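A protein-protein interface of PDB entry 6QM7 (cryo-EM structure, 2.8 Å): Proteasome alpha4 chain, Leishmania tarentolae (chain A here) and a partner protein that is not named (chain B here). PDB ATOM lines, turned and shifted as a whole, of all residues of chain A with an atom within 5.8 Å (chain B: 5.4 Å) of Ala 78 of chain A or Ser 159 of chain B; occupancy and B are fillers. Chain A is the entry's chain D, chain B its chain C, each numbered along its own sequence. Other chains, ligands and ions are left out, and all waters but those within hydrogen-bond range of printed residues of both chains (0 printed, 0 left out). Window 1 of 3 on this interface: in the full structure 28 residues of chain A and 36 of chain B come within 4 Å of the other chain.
The side-chain carboxylate (OD1) of Asp 79 of chain A lies within hydrogen-bond range of the side-chain amide nitrogen (NE2) of Gln 125 of chain B.
The guanidinium group (NH2) of Arg 81 of chain A sits at hydrogen-bond distance from the backbone carbonyl oxygen (O) of Gly 160 of chain B (2.5 Å).
OG of Ser 159 of chain B sits at hydrogen-bond distance from OD2 of Asp 161 of chain B (2.7 Å).
O of Gly 160 of chain B lies close to SG of Cys 121 of chain B (3.5 Å).
The side-chain hydroxyl of Thr 128 of chain B sits at hydrogen-bond distance from the backbone carbonyl oxygen of Gln 125 of chain B, at 2.7 Å.
The side-chain hydroxyl (OG) of Ser 159 of chain B lies within hydrogen-bond range of the side-chain carboxylate (OE1) of Glu 157 of chain B.
Ser 77 of chain A touches Asp 161 of chain B.
Gln 125 of chain B touches Ala 78 of chain A (CG to CB, 3.7 Å).
CB of Ala 78 of chain A touches O of Ser 159 of chain B, at 3.4 Å.
Ala 78 of chain A touches Gly 160 of chain B.
Asp 161 of chain B touches Ala 78 of chain A (N to CB, 3.8 Å).
Arg 81 of chain A touches Cys 121 of chain B (NH1 to O, 3.7 Å).
Asp 161 of chain B touches Arg 81 of chain A (N to NH2, 3.8 Å).
Gln 125 of chain B touches Val 82 of chain A.
Of the printed residues of chain B, Ser 77 of chain A touches Asp 161 (3.9 Å).
Of chain B, only Gln 125 (3.7 Å), Ser 159 (3.4 Å), Gly 160 (3.96 Å) and Asp 161 (3.8 Å) come within 4 Å of Ala 78 of chain A.
Printed residues of chain A within 4 Å of Gln 125 of chain B: Ala 78, Asp 79 and Val 82.
Of chain A, only Ala 78 comes within 4 Å of Ser 159 of chain B.
The nearest printed residue of chain B that does not touch Ala 78 of chain A is Cys 121 of chain B (5.8 Å).
The nearest residue of chain A that does not touch Ser 159 of chain B is Asp 79 of chain A (5.5 Å).
Of the 10 printed residues of chain B, 5 touch a printed residue of chain A.
Hydrophobic or aromatic side chains of chain A within 4 Å of the printed part of chain B: Ala 78 and Val 82.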
ATOM      1  N   LEU A  76      13.872  17.550  -6.049  1.00  0.00           N
ATOM      2  CA  LEU A  76      13.224  16.684  -7.067  1.00  0.00           C
ATOM      3  C   LEU A  76      14.264  15.712  -7.635  1.00  0.00           C
ATOM      4  O   LEU A  76      15.196  16.164  -8.335  1.00  0.00           O
ATOM      5  CB  LEU A  76      12.594  17.558  -8.155  1.00  0.00           C
ATOM      6  CG  LEU A  76      11.642  18.663  -7.682  1.00  0.00           C
ATOM      7  CD1 LEU A  76      11.129  19.454  -8.882  1.00  0.00           C
ATOM      8  CD2 LEU A  76      10.482  18.103  -6.860  1.00  0.00           C
ATOM      9  N   SER A  77      14.094  14.425  -7.321  1.00  0.00           N
ATOM     10  CA  SER A  77      14.920  13.283  -7.798  1.00  0.00           C
ATOM     11  C   SER A  77      15.194  13.399  -9.300  1.00  0.00           C
ATOM     12  O   SER A  77      16.351  13.171  -9.703  1.00  0.00           O
ATOM     13  CB  SER A  77      14.248  11.964  -7.473  1.00  0.00           C
ATOM     14  OG  SER A  77      14.340  11.674  -6.083  1.00  0.00           O
ATOM     15  N   ALA A  78      14.155  13.719 -10.078  1.00  0.00           N
ATOM     16  CA  ALA A  78      14.167  13.778 -11.558  1.00  0.00           C
ATOM     17  C   ALA A  78      15.107  14.891 -12.027  1.00  0.00           C
ATOM     18  O   ALA A  78      15.976  14.632 -12.885  1.00  0.00           O
ATOM     19  CB  ALA A  78      12.770  14.017 -12.063  1.00  0.00           C
ATOM     20  N   ASP A  79      14.912  16.089 -11.479  1.00  0.00           N
ATOM     21  CA  ASP A  79      15.718  17.297 -11.781  1.00  0.00           C
ATOM     22  C   ASP A  79      17.172  17.044 -11.394  1.00  0.00           C
ATOM     23  O   ASP A  79      18.061  17.428 -12.168  1.00  0.00           O
ATOM     24  CB  ASP A  79      15.172  18.515 -11.035  1.00  0.00           C
ATOM     25  CG  ASP A  79      13.862  19.041 -11.595  1.00  0.00           C
ATOM     26  OD1 ASP A  79      13.120  18.248 -12.232  1.00  0.00           O
ATOM     27  OD2 ASP A  79      13.593  20.245 -11.393  1.00  0.00           O
ATOM     28  N   ALA A  80      17.393  16.448 -10.222  1.00  0.00           N
ATOM     29  CA  ALA A  80      18.743  16.176  -9.681  1.00  0.00           C
ATOM     30  C   ALA A  80      19.484  15.234 -10.625  1.00  0.00           C
ATOM     31  O   ALA A  80      20.643  15.505 -10.912  1.00  0.00           O
ATOM     32  CB  ALA A  80      18.647  15.589  -8.309  1.00  0.00           C
ATOM     33  N   ARG A  81      18.812  14.187 -11.103  1.00  0.00           N
ATOM     34  CA  ARG A  81      19.392  13.216 -12.064  1.00  0.00           C
ATOM     35  C   ARG A  81      19.911  13.962 -13.294  1.00  0.00           C
ATOM     36  O   ARG A  81      20.955  13.549 -13.830  1.00  0.00           O
ATOM     37  CB  ARG A  81      18.391  12.144 -12.497  1.00  0.00           C
ATOM     38  CG  ARG A  81      19.069  10.907 -13.074  1.00  0.00           C
ATOM     39  CD  ARG A  81      18.201  10.118 -14.041  1.00  0.00           C
ATOM     40  NE  ARG A  81      16.805  10.047 -13.612  1.00  0.00           N
ATOM     41  CZ  ARG A  81      15.756  10.602 -14.225  1.00  0.00           C
ATOM     42  NH1 ARG A  81      15.879  11.297 -15.347  1.00  0.00           N
ATOM     43  NH2 ARG A  81      14.558  10.450 -13.698  1.00  0.00           N
ATOM     44  N   VAL A  82      19.214  15.014 -13.711  1.00  0.00           N
ATOM     45  CA  VAL A  82      19.552  15.788 -14.936  1.00  0.00           C
ATOM     46  C   VAL A  82      20.773  16.666 -14.664  1.00  0.00           C
ATOM     47  O   VAL A  82      21.639  16.718 -15.558  1.00  0.00           O
ATOM     48  CB  VAL A  82      18.336  16.588 -15.431  1.00  0.00           C
ATOM     49  CG1 VAL A  82      18.726  17.695 -16.398  1.00  0.00           C
ATOM     50  CG2 VAL A  82      17.319  15.645 -16.055  1.00  0.00           C
ATOM     51  N   LEU A  83      20.832  17.332 -13.508  1.00  0.00           N
ATOM     52  CA  LEU A  83      22.024  18.093 -13.039  1.00  0.00           C
ATOM     53  C   LEU A  83      23.238  17.169 -12.950  1.00  0.00           C
ATOM     54  O   LEU A  83      24.310  17.547 -13.436  1.00  0.00           O
ATOM     55  CB  LEU A  83      21.767  18.669 -11.648  1.00  0.00           C
ATOM     56  CG  LEU A  83      21.126  20.045 -11.604  1.00  0.00           C
ATOM     57  CD1 LEU A  83      20.994  20.482 -10.156  1.00  0.00           C
ATOM     58  CD2 LEU A  83      21.950  21.045 -12.402  1.00  0.00           C
ATOM     59  N   VAL B  21       2.208  17.599 -13.026  1.00  0.00           N
ATOM     60  CA  VAL B  21       2.716  16.227 -12.717  1.00  0.00           C
ATOM     61  C   VAL B  21       1.813  15.575 -11.667  1.00  0.00           C
ATOM     62  O   VAL B  21       1.422  14.435 -11.877  1.00  0.00           O
ATOM     63  CB  VAL B  21       4.198  16.246 -12.289  1.00  0.00           C
ATOM     64  CG1 VAL B  21       4.629  14.941 -11.635  1.00  0.00           C
ATOM     65  CG2 VAL B  21       5.115  16.571 -13.465  1.00  0.00           C
ATOM     66  N   CYS B 121      12.942   8.122 -18.751  1.00  0.00           N
ATOM     67  CA  CYS B 121      12.572   9.021 -17.633  1.00  0.00           C
ATOM     68  C   CYS B 121      13.224  10.399 -17.761  1.00  0.00           C
ATOM     69  O   CYS B 121      12.680  11.341 -17.189  1.00  0.00           O
ATOM     70  CB  CYS B 121      12.946   8.364 -16.321  1.00  0.00           C
ATOM     71  SG  CYS B 121      11.809   7.013 -15.936  1.00  0.00           S
ATOM     72  N   LYS B 124      10.616  12.063 -20.003  1.00  0.00           N
ATOM     73  CA  LYS B 124       9.459  12.492 -19.181  1.00  0.00           C
ATOM     74  C   LYS B 124       9.819  13.738 -18.368  1.00  0.00           C
ATOM     75  O   LYS B 124       8.935  14.598 -18.205  1.00  0.00           O
ATOM     76  CB  LYS B 124       9.007  11.340 -18.287  1.00  0.00           C
ATOM     77  CG  LYS B 124       8.444  10.164 -19.067  1.00  0.00           C
ATOM     78  CD  LYS B 124       7.156   9.587 -18.510  1.00  0.00           C
ATOM     79  CE  LYS B 124       7.393   8.338 -17.702  1.00  0.00           C
ATOM     80  NZ  LYS B 124       8.357   8.643 -16.623  1.00  0.00           N
ATOM     81  N   GLN B 125      11.047  13.826 -17.859  1.00  0.00           N
ATOM     82  CA  GLN B 125      11.485  14.939 -16.977  1.00  0.00           C
ATOM     83  C   GLN B 125      11.419  16.236 -17.778  1.00  0.00           C
ATOM     84  O   GLN B 125      10.860  17.212 -17.243  1.00  0.00           O
ATOM     85  CB  GLN B 125      12.894  14.701 -16.426  1.00  0.00           C
ATOM     86  CG  GLN B 125      13.299  15.683 -15.334  1.00  0.00           C
ATOM     87  CD  GLN B 125      13.845  16.992 -15.852  1.00  0.00           C
ATOM     88  OE1 GLN B 125      14.468  17.058 -16.913  1.00  0.00           O
ATOM     89  NE2 GLN B 125      13.617  18.050 -15.089  1.00  0.00           N
ATOM     90  N   THR B 128       8.360  18.361 -17.813  1.00  0.00           N
ATOM     91  CA  THR B 128       8.016  18.987 -16.513  1.00  0.00           C
ATOM     92  C   THR B 128       8.874  20.223 -16.252  1.00  0.00           C
ATOM     93  O   THR B 128       8.666  20.825 -15.176  1.00  0.00           O
ATOM     94  CB  THR B 128       8.222  18.025 -15.339  1.00  0.00           C
ATOM     95  OG1 THR B 128       9.597  17.948 -14.960  1.00  0.00           O
ATOM     96  CG2 THR B 128       7.736  16.631 -15.661  1.00  0.00           C
ATOM     97  N   GLU B 157       7.698   7.254 -13.240  1.00  0.00           N
ATOM     98  CA  GLU B 157       6.653   8.194 -12.768  1.00  0.00           C
ATOM     99  C   GLU B 157       6.605   9.361 -13.756  1.00  0.00           C
ATOM    100  O   GLU B 157       7.617   9.676 -14.360  1.00  0.00           O
ATOM    101  CB  GLU B 157       6.986   8.576 -11.320  1.00  0.00           C
ATOM    102  CG  GLU B 157       5.795   8.536 -10.367  1.00  0.00           C
ATOM    103  CD  GLU B 157       5.623   9.752  -9.459  1.00  0.00           C
ATOM    104  OE1 GLU B 157       5.754  10.908  -9.959  1.00  0.00           O
ATOM    105  OE2 GLU B 157       5.337   9.549  -8.256  1.00  0.00           O
ATOM    106  N   PRO B 158       5.466  10.057 -13.954  1.00  0.00           N
ATOM    107  CA  PRO B 158       5.391  11.163 -14.912  1.00  0.00           C
ATOM    108  C   PRO B 158       6.388  12.310 -14.679  1.00  0.00           C
ATOM    109  O   PRO B 158       6.751  12.987 -15.637  1.00  0.00           O
ATOM    110  CB  PRO B 158       3.998  11.760 -14.684  1.00  0.00           C
ATOM    111  CG  PRO B 158       3.213  10.642 -14.056  1.00  0.00           C
ATOM    112  CD  PRO B 158       4.208   9.865 -13.224  1.00  0.00           C
ATOM    113  N   SER B 159       6.758  12.523 -13.410  1.00  0.00           N
ATOM    114  CA  SER B 159       7.806  13.469 -12.942  1.00  0.00           C
ATOM    115  C   SER B 159       9.113  13.222 -13.687  1.00  0.00           C
ATOM    116  O   SER B 159       9.864  14.188 -13.895  1.00  0.00           O
ATOM    117  CB  SER B 159       8.038  13.338 -11.461  1.00  0.00           C
ATOM    118  OG  SER B 159       8.005  11.976 -11.082  1.00  0.00           O
ATOM    119  N   GLY B 160       9.385  11.964 -14.017  1.00  0.00           N
ATOM    120  CA  GLY B 160      10.696  11.507 -14.493  1.00  0.00           C
ATOM    121  C   GLY B 160      11.361  10.598 -13.476  1.00  0.00           C
ATOM    122  O   GLY B 160      12.199   9.816 -13.912  1.00  0.00           O
ATOM    123  N   ASP B 161      11.032  10.670 -12.177  1.00  0.00           N
ATOM    124  CA  ASP B 161      11.720   9.807 -11.179  1.00  0.00           C
ATOM    125  C   ASP B 161      11.287   8.367 -11.427  1.00  0.00           C
ATOM    126  O   ASP B 161      10.138   8.163 -11.807  1.00  0.00           O
ATOM    127  CB  ASP B 161      11.565  10.201  -9.704  1.00  0.00           C
ATOM    128  CG  ASP B 161      10.304  10.954  -9.310  1.00  0.00           C
ATOM    129  OD1 ASP B 161       9.395  10.312  -8.728  1.00  0.00           O
ATOM    130  OD2 ASP B 161      10.257  12.190  -9.550  1.00  0.00           O
